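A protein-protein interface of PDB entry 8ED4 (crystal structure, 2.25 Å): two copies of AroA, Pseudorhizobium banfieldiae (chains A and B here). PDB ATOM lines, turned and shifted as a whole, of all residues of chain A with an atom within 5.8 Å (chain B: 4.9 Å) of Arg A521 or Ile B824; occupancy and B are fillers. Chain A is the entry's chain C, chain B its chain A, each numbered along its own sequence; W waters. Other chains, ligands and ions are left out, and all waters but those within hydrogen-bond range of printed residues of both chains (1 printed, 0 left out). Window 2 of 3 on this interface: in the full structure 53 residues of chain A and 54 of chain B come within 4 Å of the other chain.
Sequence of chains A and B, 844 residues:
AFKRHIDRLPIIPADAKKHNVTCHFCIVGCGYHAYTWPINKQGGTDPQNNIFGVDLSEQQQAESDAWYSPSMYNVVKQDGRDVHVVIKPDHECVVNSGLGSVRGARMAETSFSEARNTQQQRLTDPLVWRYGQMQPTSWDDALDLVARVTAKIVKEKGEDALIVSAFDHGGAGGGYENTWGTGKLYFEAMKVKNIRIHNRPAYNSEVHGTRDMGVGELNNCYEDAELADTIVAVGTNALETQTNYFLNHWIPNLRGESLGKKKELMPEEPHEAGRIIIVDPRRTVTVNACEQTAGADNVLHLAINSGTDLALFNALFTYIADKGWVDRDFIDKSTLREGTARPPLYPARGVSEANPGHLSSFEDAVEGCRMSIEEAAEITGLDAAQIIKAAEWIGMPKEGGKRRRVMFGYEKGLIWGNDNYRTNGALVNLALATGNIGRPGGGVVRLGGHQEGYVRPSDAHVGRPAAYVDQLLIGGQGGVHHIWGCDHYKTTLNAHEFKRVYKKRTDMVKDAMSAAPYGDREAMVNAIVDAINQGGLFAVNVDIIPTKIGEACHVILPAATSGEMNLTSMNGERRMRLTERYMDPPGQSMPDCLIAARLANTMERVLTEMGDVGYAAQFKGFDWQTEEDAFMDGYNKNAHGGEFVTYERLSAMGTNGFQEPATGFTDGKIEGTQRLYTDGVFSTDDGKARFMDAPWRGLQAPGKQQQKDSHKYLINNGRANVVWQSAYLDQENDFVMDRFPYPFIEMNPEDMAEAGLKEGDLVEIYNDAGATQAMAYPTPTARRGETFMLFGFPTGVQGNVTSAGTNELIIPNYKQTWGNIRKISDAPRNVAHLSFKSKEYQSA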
ATOM      1  N   ARG A 130      27.634 -24.979  13.287  1.00  0.00           N
ATOM      2  CA  ARG A 130      27.356 -23.562  13.600  1.00  0.00           C
ATOM      3  C   ARG A 130      28.468 -23.006  14.485  1.00  0.00           C
ATOM      4  O   ARG A 130      29.158 -23.787  15.181  1.00  0.00           O
ATOM      5  CB  ARG A 130      25.997 -23.420  14.283  1.00  0.00           C
ATOM      6  CG  ARG A 130      25.832 -24.189  15.584  1.00  0.00           C
ATOM      7  CD  ARG A 130      24.409 -23.971  16.073  1.00  0.00           C
ATOM      8  NE  ARG A 130      24.157 -24.605  17.364  1.00  0.00           N
ATOM      9  CZ  ARG A 130      23.142 -25.404  17.651  1.00  0.00           C
ATOM     10  NH1 ARG A 130      22.231 -25.699  16.741  1.00  0.00           N
ATOM     11  NH2 ARG A 130      23.029 -25.888  18.870  1.00  0.00           N
ATOM     12  N   TYR A 131      28.646 -21.694  14.449  1.00  0.00           N
ATOM     13  CA  TYR A 131      29.671 -20.992  15.252  1.00  0.00           C
ATOM     14  C   TYR A 131      31.075 -21.452  14.826  1.00  0.00           C
ATOM     15  O   TYR A 131      31.993 -21.256  15.609  1.00  0.00           O
ATOM     16  CB  TYR A 131      29.357 -21.219  16.737  1.00  0.00           C
ATOM     17  CG  TYR A 131      27.909 -20.990  17.091  1.00  0.00           C
ATOM     18  CD1 TYR A 131      27.188 -19.929  16.557  1.00  0.00           C
ATOM     19  CD2 TYR A 131      27.248 -21.831  17.972  1.00  0.00           C
ATOM     20  CE1 TYR A 131      25.855 -19.718  16.885  1.00  0.00           C
ATOM     21  CE2 TYR A 131      25.925 -21.622  18.331  1.00  0.00           C
ATOM     22  CZ  TYR A 131      25.222 -20.565  17.785  1.00  0.00           C
ATOM     23  OH  TYR A 131      23.915 -20.386  18.140  1.00  0.00           O
ATOM     24  N   THR A 137      23.517 -30.416  19.862  1.00  0.00           N
ATOM     25  CA  THR A 137      22.238 -29.712  20.039  1.00  0.00           C
ATOM     26  C   THR A 137      21.191 -30.733  20.451  1.00  0.00           C
ATOM     27  O   THR A 137      21.559 -31.880  20.710  1.00  0.00           O
ATOM     28  CB  THR A 137      21.898 -28.909  18.778  1.00  0.00           C
ATOM     29  OG1 THR A 137      20.864 -27.999  19.151  1.00  0.00           O
ATOM     30  CG2 THR A 137      21.475 -29.758  17.601  1.00  0.00           C
ATOM     31  N   ASP A 141      15.778 -29.309  17.739  1.00  0.00           N
ATOM     32  CA  ASP A 141      16.541 -28.293  16.973  1.00  0.00           C
ATOM     33  C   ASP A 141      17.075 -28.933  15.688  1.00  0.00           C
ATOM     34  O   ASP A 141      16.773 -28.415  14.627  1.00  0.00           O
ATOM     35  CB  ASP A 141      17.669 -27.677  17.797  1.00  0.00           C
ATOM     36  CG  ASP A 141      18.522 -26.689  17.024  1.00  0.00           C
ATOM     37  OD1 ASP A 141      17.961 -25.882  16.269  1.00  0.00           O
ATOM     38  OD2 ASP A 141      19.757 -26.744  17.185  1.00  0.00           O
ATOM     39  N   ASP A 144      14.332 -30.000  13.133  1.00  0.00           N
ATOM     40  CA  ASP A 144      13.717 -28.761  12.602  1.00  0.00           C
ATOM     41  C   ASP A 144      14.632 -28.209  11.492  1.00  0.00           C
ATOM     42  O   ASP A 144      14.124 -27.931  10.389  1.00  0.00           O
ATOM     43  CB  ASP A 144      13.433 -27.761  13.721  1.00  0.00           C
ATOM     44  CG  ASP A 144      12.843 -26.461  13.205  1.00  0.00           C
ATOM     45  OD1 ASP A 144      11.607 -26.429  12.939  1.00  0.00           O
ATOM     46  OD2 ASP A 144      13.632 -25.504  13.031  1.00  0.00           O
ATOM     47  N   LEU A 145      15.937 -28.080  11.739  1.00  0.00           N
ATOM     48  CA  LEU A 145      16.846 -27.554  10.688  1.00  0.00           C
ATOM     49  C   LEU A 145      16.784 -28.462   9.446  1.00  0.00           C
ATOM     50  O   LEU A 145      16.635 -27.924   8.322  1.00  0.00           O
ATOM     51  CB  LEU A 145      18.275 -27.446  11.220  1.00  0.00           C
ATOM     52  CG  LEU A 145      19.301 -26.956  10.199  1.00  0.00           C
ATOM     53  CD1 LEU A 145      18.969 -25.550   9.728  1.00  0.00           C
ATOM     54  CD2 LEU A 145      20.701 -27.008  10.778  1.00  0.00           C
ATOM     55  N   ARG A 148      13.426 -28.112   7.572  1.00  0.00           N
ATOM     56  CA  ARG A 148      13.212 -26.771   6.968  1.00  0.00           C
ATOM     57  C   ARG A 148      14.045 -26.664   5.678  1.00  0.00           C
ATOM     58  O   ARG A 148      13.480 -26.246   4.651  1.00  0.00           O
ATOM     59  CB  ARG A 148      13.511 -25.652   7.969  1.00  0.00           C
ATOM     60  CG  ARG A 148      12.426 -25.476   9.023  1.00  0.00           C
ATOM     61  CD  ARG A 148      12.506 -24.163   9.799  1.00  0.00           C
ATOM     62  NE  ARG A 148      11.618 -24.264  10.957  1.00  0.00           N
ATOM     63  CZ  ARG A 148      10.282 -24.065  10.954  1.00  0.00           C
ATOM     64  NH1 ARG A 148       9.644 -23.660   9.861  1.00  0.00           N
ATOM     65  NH2 ARG A 148       9.590 -24.247  12.074  1.00  0.00           N
ATOM     66  N   PRO A 517      23.269 -15.802  11.010  1.00  0.00           N
ATOM     67  CA  PRO A 517      22.808 -15.910  12.397  1.00  0.00           C
ATOM     68  C   PRO A 517      22.050 -17.232  12.603  1.00  0.00           C
ATOM     69  O   PRO A 517      21.142 -17.480  11.856  1.00  0.00           O
ATOM     70  CB  PRO A 517      21.890 -14.684  12.610  1.00  0.00           C
ATOM     71  CG  PRO A 517      21.797 -13.971  11.250  1.00  0.00           C
ATOM     72  CD  PRO A 517      22.433 -14.881  10.217  1.00  0.00           C
ATOM     73  N   TYR A 518      22.424 -18.060  13.585  1.00  0.00           N
ATOM     74  CA  TYR A 518      21.740 -19.364  13.810  1.00  0.00           C
ATOM     75  C   TYR A 518      20.452 -19.167  14.627  1.00  0.00           C
ATOM     76  O   TYR A 518      19.411 -19.751  14.243  1.00  0.00           O
ATOM     77  CB  TYR A 518      22.653 -20.413  14.452  1.00  0.00           C
ATOM     78  CG  TYR A 518      21.991 -21.769  14.497  1.00  0.00           C
ATOM     79  CD1 TYR A 518      21.172 -22.125  15.557  1.00  0.00           C
ATOM     80  CD2 TYR A 518      22.099 -22.657  13.436  1.00  0.00           C
ATOM     81  CE1 TYR A 518      20.518 -23.347  15.589  1.00  0.00           C
ATOM     82  CE2 TYR A 518      21.449 -23.879  13.449  1.00  0.00           C
ATOM     83  CZ  TYR A 518      20.656 -24.227  14.529  1.00  0.00           C
ATOM     84  OH  TYR A 518      20.012 -25.431  14.561  1.00  0.00           O
ATOM     85  N   GLY A 519      20.515 -18.384  15.708  1.00  0.00           N
ATOM     86  CA  GLY A 519      19.406 -18.140  16.654  1.00  0.00           C
ATOM     87  C   GLY A 519      18.174 -17.559  15.971  1.00  0.00           C
ATOM     88  O   GLY A 519      17.072 -17.700  16.539  1.00  0.00           O
ATOM     89  N   ASP A 520      18.351 -16.929  14.806  1.00  0.00           N
ATOM     90  CA  ASP A 520      17.272 -16.624  13.823  1.00  0.00           C
ATOM     91  C   ASP A 520      17.264 -17.693  12.715  1.00  0.00           C
ATOM     92  O   ASP A 520      18.030 -17.546  11.725  1.00  0.00           O
ATOM     93  CB  ASP A 520      17.438 -15.216  13.243  1.00  0.00           C
ATOM     94  CG  ASP A 520      16.451 -14.903  12.138  1.00  0.00           C
ATOM     95  OD1 ASP A 520      15.376 -15.545  12.107  1.00  0.00           O
ATOM     96  OD2 ASP A 520      16.772 -14.030  11.311  1.00  0.00           O
ATOM     97  N   ARG A 521      16.419 -18.720  12.858  1.00  0.00           N
ATOM     98  CA  ARG A 521      16.533 -19.969  12.060  1.00  0.00           C
ATOM     99  C   ARG A 521      16.253 -19.655  10.586  1.00  0.00           C
ATOM    100  O   ARG A 521      16.994 -20.172   9.736  1.00  0.00           O
ATOM    101  CB  ARG A 521      15.642 -21.090  12.610  1.00  0.00           C
ATOM    102  CG  ARG A 521      16.254 -22.480  12.459  1.00  0.00           C
ATOM    103  CD  ARG A 521      17.413 -22.784  13.414  1.00  0.00           C
ATOM    104  NE  ARG A 521      16.947 -23.205  14.744  1.00  0.00           N
ATOM    105  CZ  ARG A 521      17.080 -22.530  15.894  1.00  0.00           C
ATOM    106  NH1 ARG A 521      17.708 -21.365  15.936  1.00  0.00           N
ATOM    107  NH2 ARG A 521      16.585 -23.044  17.013  1.00  0.00           N
ATOM    108  N   GLU A 522      15.247 -18.824  10.301  1.00  0.00           N
ATOM    109  CA  GLU A 522      14.799 -18.540   8.915  1.00  0.00           C
ATOM    110  C   GLU A 522      15.959 -17.955   8.099  1.00  0.00           C
ATOM    111  O   GLU A 522      16.051 -18.268   6.898  1.00  0.00           O
ATOM    112  CB  GLU A 522      13.600 -17.593   8.882  1.00  0.00           C
ATOM    113  CG  GLU A 522      12.899 -17.603   7.528  1.00  0.00           C
ATOM    114  CD  GLU A 522      11.766 -16.604   7.326  1.00  0.00           C
ATOM    115  OE1 GLU A 522      11.037 -16.739   6.298  1.00  0.00           O
ATOM    116  OE2 GLU A 522      11.614 -15.693   8.180  1.00  0.00           O
ATOM    117  N   ALA A 523      16.812 -17.132   8.707  1.00  0.00           N
ATOM    118  CA  ALA A 523      17.963 -16.516   8.012  1.00  0.00           C
ATOM    119  C   ALA A 523      19.012 -17.596   7.733  1.00  0.00           C
ATOM    120  O   ALA A 523      19.603 -17.585   6.632  1.00  0.00           O
ATOM    121  CB  ALA A 523      18.533 -15.392   8.839  1.00  0.00           C
ATOM    122  N   MET A 524      19.230 -18.498   8.692  1.00  0.00           N
ATOM    123  CA  MET A 524      20.136 -19.666   8.543  1.00  0.00           C
ATOM    124  C   MET A 524      19.675 -20.498   7.343  1.00  0.00           C
ATOM    125  O   MET A 524      20.494 -20.733   6.449  1.00  0.00           O
ATOM    126  CB  MET A 524      20.144 -20.531   9.807  1.00  0.00           C
ATOM    127  CG  MET A 524      21.019 -21.758   9.703  1.00  0.00           C
ATOM    128  SD  MET A 524      22.669 -21.331   9.135  1.00  0.00           S
ATOM    129  CE  MET A 524      23.305 -20.502  10.592  1.00  0.00           C
ATOM    130  N   VAL A 525      18.388 -20.845   7.297  1.00  0.00           N
ATOM    131  CA  VAL A 525      17.771 -21.637   6.194  1.00  0.00           C
ATOM    132  C   VAL A 525      18.020 -20.930   4.854  1.00  0.00           C
ATOM    133  O   VAL A 525      18.415 -21.614   3.911  1.00  0.00           O
ATOM    134  CB  VAL A 525      16.278 -21.922   6.447  1.00  0.00           C
ATOM    135  CG1 VAL A 525      15.631 -22.609   5.251  1.00  0.00           C
ATOM    136  CG2 VAL A 525      16.071 -22.757   7.704  1.00  0.00           C
ATOM    137  N   ASN A 526      17.832 -19.616   4.768  1.00  0.00           N
ATOM    138  CA  ASN A 526      17.889 -18.854   3.486  1.00  0.00           C
ATOM    139  C   ASN A 526      19.344 -18.785   2.997  1.00  0.00           C
ATOM    140  O   ASN A 526      19.571 -18.861   1.781  1.00  0.00           O
ATOM    141  CB  ASN A 526      17.271 -17.453   3.632  1.00  0.00           C
ATOM    142  CG  ASN A 526      15.759 -17.456   3.755  1.00  0.00           C
ATOM    143  OD1 ASN A 526      15.067 -18.151   3.023  1.00  0.00           O
ATOM    144  ND2 ASN A 526      15.218 -16.635   4.634  1.00  0.00           N
ATOM    145  N   LEU B 762      19.405 -24.570  26.107  1.00  0.00           N
ATOM    146  CA  LEU B 762      20.493 -24.199  25.176  1.00  0.00           C
ATOM    147  C   LEU B 762      20.196 -22.774  24.713  1.00  0.00           C
ATOM    148  O   LEU B 762      19.110 -22.556  24.122  1.00  0.00           O
ATOM    149  CB  LEU B 762      20.530 -25.211  24.026  1.00  0.00           C
ATOM    150  CG  LEU B 762      21.774 -25.209  23.134  1.00  0.00           C
ATOM    151  CD1 LEU B 762      23.061 -25.069  23.932  1.00  0.00           C
ATOM    152  CD2 LEU B 762      21.833 -26.490  22.317  1.00  0.00           C
ATOM    153  N   VAL B 763      21.097 -21.834  25.004  1.00  0.00           N
ATOM    154  CA  VAL B 763      20.936 -20.407  24.614  1.00  0.00           C
ATOM    155  C   VAL B 763      22.034 -20.043  23.613  1.00  0.00           C
ATOM    156  O   VAL B 763      23.129 -20.618  23.687  1.00  0.00           O
ATOM    157  CB  VAL B 763      20.940 -19.477  25.837  1.00  0.00           C
ATOM    158  CG1 VAL B 763      19.823 -19.836  26.800  1.00  0.00           C
ATOM    159  CG2 VAL B 763      22.279 -19.468  26.558  1.00  0.00           C
ATOM    160  N   GLU B 764      21.722 -19.120  22.705  1.00  0.00           N
ATOM    161  CA  GLU B 764      22.734 -18.426  21.883  1.00  0.00           C
ATOM    162  C   GLU B 764      23.132 -17.126  22.577  1.00  0.00           C
ATOM    163  O   GLU B 764      22.223 -16.359  22.957  1.00  0.00           O
ATOM    164  CB  GLU B 764      22.187 -18.094  20.506  1.00  0.00           C
ATOM    165  CG  GLU B 764      23.240 -17.555  19.573  1.00  0.00           C
ATOM    166  CD  GLU B 764      22.587 -17.322  18.238  1.00  0.00           C
ATOM    167  OE1 GLU B 764      21.877 -16.309  18.129  1.00  0.00           O
ATOM    168  OE2 GLU B 764      22.698 -18.201  17.361  1.00  0.00           O
ATOM    169  N   GLN B 773      26.993 -20.832  21.869  1.00  0.00           N
ATOM    170  CA  GLN B 773      25.952 -21.519  22.659  1.00  0.00           C
ATOM    171  C   GLN B 773      26.498 -21.860  24.035  1.00  0.00           C
ATOM    172  O   GLN B 773      27.719 -22.075  24.166  1.00  0.00           O
ATOM    173  CB  GLN B 773      25.474 -22.792  21.964  1.00  0.00           C
ATOM    174  CG  GLN B 773      26.566 -23.829  21.712  1.00  0.00           C
ATOM    175  CD  GLN B 773      26.000 -25.070  21.059  1.00  0.00           C
ATOM    176  OE1 GLN B 773      25.054 -24.998  20.284  1.00  0.00           O
ATOM    177  NE2 GLN B 773      26.563 -26.223  21.383  1.00  0.00           N
ATOM    178  N   ARG B 822      19.432 -15.439  23.652  1.00  0.00           N
ATOM    179  CA  ARG B 822      18.124 -15.963  23.203  1.00  0.00           C
ATOM    180  C   ARG B 822      18.197 -17.492  23.181  1.00  0.00           C
ATOM    181  O   ARG B 822      19.273 -18.058  22.919  1.00  0.00           O
ATOM    182  CB  ARG B 822      17.742 -15.397  21.835  1.00  0.00           C
ATOM    183  CG  ARG B 822      18.734 -15.724  20.732  1.00  0.00           C
ATOM    184  CD  ARG B 822      18.330 -15.022  19.455  1.00  0.00           C
ATOM    185  NE  ARG B 822      19.372 -15.050  18.438  1.00  0.00           N
ATOM    186  CZ  ARG B 822      19.431 -14.218  17.399  1.00  0.00           C
ATOM    187  NH1 ARG B 822      18.523 -13.271  17.227  1.00  0.00           N
ATOM    188  NH2 ARG B 822      20.420 -14.310  16.533  1.00  0.00           N
ATOM    189  N   LYS B 823      17.073 -18.126  23.474  1.00  0.00           N
ATOM    190  CA  LYS B 823      16.933 -19.595  23.489  1.00  0.00           C
ATOM    191  C   LYS B 823      17.180 -20.135  22.079  1.00  0.00           C
ATOM    192  O   LYS B 823      16.661 -19.541  21.127  1.00  0.00           O
ATOM    193  CB  LYS B 823      15.556 -20.013  24.006  1.00  0.00           C
ATOM    194  CG  LYS B 823      15.415 -21.523  24.157  1.00  0.00           C
ATOM    195  CD  LYS B 823      14.398 -21.947  25.188  1.00  0.00           C
ATOM    196  CE  LYS B 823      12.976 -21.635  24.772  1.00  0.00           C
ATOM    197  NZ  LYS B 823      12.054 -22.690  25.272  1.00  0.00           N
ATOM    198  N   ILE B 824      17.951 -21.221  21.981  1.00  0.00           N
ATOM    199  CA  ILE B 824      18.075 -22.093  20.777  1.00  0.00           C
ATOM    200  C   ILE B 824      17.065 -23.240  20.897  1.00  0.00           C
ATOM    201  O   ILE B 824      16.428 -23.613  19.907  1.00  0.00           O
ATOM    202  CB  ILE B 824      19.496 -22.667  20.688  1.00  0.00           C
ATOM    203  CG1 ILE B 824      20.545 -21.615  20.342  1.00  0.00           C
ATOM    204  CG2 ILE B 824      19.517 -23.811  19.695  1.00  0.00           C
ATOM    205  CD1 ILE B 824      21.966 -22.082  20.580  1.00  0.00           C
ATOM    206  N   SER B 825      16.987 -23.832  22.081  1.00  0.00           N
ATOM    207  CA  SER B 825      16.271 -25.102  22.334  1.00  0.00           C
ATOM    208  C   SER B 825      15.953 -25.235  23.827  1.00  0.00           C
ATOM    209  O   SER B 825      16.753 -24.764  24.648  1.00  0.00           O
ATOM    210  CB  SER B 825      17.111 -26.251  21.849  1.00  0.00           C
ATOM    211  OG  SER B 825      16.679 -27.471  22.424  1.00  0.00           O
ATOM    212  N   ASP B 826      14.827 -25.870  24.154  1.00  0.00           N
ATOM    213  CA  ASP B 826      14.538 -26.356  25.524  1.00  0.00           C
ATOM    214  C   ASP B 826      15.681 -27.277  25.938  1.00  0.00           C
ATOM    215  O   ASP B 826      16.317 -27.849  25.025  1.00  0.00           O
ATOM    216  CB  ASP B 826      13.207 -27.093  25.598  1.00  0.00           C
ATOM    217  CG  ASP B 826      12.013 -26.171  25.443  1.00  0.00           C
ATOM    218  OD1 ASP B 826      11.933 -25.187  26.203  1.00  0.00           O
ATOM    219  OD2 ASP B 826      11.183 -26.441  24.573  1.00  0.00           O
HETATM  220  O   HOH W   1      24.069 -16.776  15.365  1.00  0.00           O
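The guanidinium group (NH2) of Arg A521 lies within hydrogen-bond range of the backbone carbonyl oxygen (O) of Ile B824 (3.0 Å). OE2 of Glu B764 lies within hydrogen-bond range of N of Gly A519, at 2.7 Å. The guanidinium group of Arg A130 lies within hydrogen-bond range of the side-chain amide oxygen of Gln B773 (2.6 Å). The side-chain hydroxyl (OH) of Tyr A131 sits at hydrogen-bond distance from the side-chain carboxylate (OE2) of Glu B764 (2.6 Å).
N of Leu B762 is in hydrogen-bond range of O of Ser B825 (3.0 Å). OE1 of Glu B764 is in salt-bridge range of NE of Arg B822. NH1 of Arg A130 is in salt-bridge range of OD2 of Asp A141. The side-chain carboxylate of Asp A141 is in hydrogen-bond range of the side-chain hydroxyl of Tyr A518 (2.7 Å). O of Leu B762 is in hydrogen-bond range of N of Ile B824, 2.8 Å away. The backbone carbonyl oxygen (O) of Tyr A518 sits at hydrogen-bond distance from the guanidinium group (NH1) of Arg A521.
Of the 17 printed residues of chain A, 8 touch a printed residue of chain B. Printed residues of chain A that touch a printed residue of chain B: Arg A130, Tyr A131, Thr A137, Asp A141, Tyr A518, Gly A519, Asp A520 and Arg A521. Hydrophobic or aromatic side chains of chain A that line the printed part of chain B: Tyr A131 and Tyr A518. Among the printed residues, 12 pairs touch across the chains. Among the printed residues, no Asp or Glu carboxylate lies within 4 Å of a Lys or Arg side-chain nitrogen of the other chain.
Water W1 bridges N of Tyr A518 (2.7 Å) and OE2 of Glu B764 (2.8 Å).
Arg A521 touches just one residue of chain B: Ile B824 (3.0 Å). Of chain A, only Tyr A131, Asp A141 and Arg A521 come within 4 Å of Ile B824. Printed residues of chain A within 4 Å of Glu B764: Tyr A131, Tyr A518 and Gly A519. Of the printed residues of chain A, Leu B762 touches Arg A130 (3.7 Å) and Thr A137 (3.6 Å). Printed residues of chain B within 4 Å of Tyr A518: Glu B764 (3.7 Å). Asn A526 touches none of the printed residues of chain B. Asp B826 touches none of the printed residues of chain A. The nearest residue of chain A that does not touch Ile B824 is Arg A130 (4.2 Å). The nearest printed residue of chain B that does not touch Arg A130 is Ile B824 (4.2 Å).
Leu B762 touches Arg A130. Gln B773 touches Tyr A131. OH of Tyr A131 touches CD1 of Ile B824, at 3.6 Å. CD2 of Leu B762 touches OG1 of Thr A137, at 3.6 Å. Asp A141 touches Ile B824. CB of Tyr A518 touches OE2 of Glu B764 (3.7 Å). Gly A519 touches Arg B822 (CA to NE, 3.6 Å). Asp A520 touches Arg B822 (N to NH2, 3.8 Å).
No position is printed for both chains. Of the 12 pairs that touch across the chains among the printed residues, none has its exchanged pair printed and touching as well.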
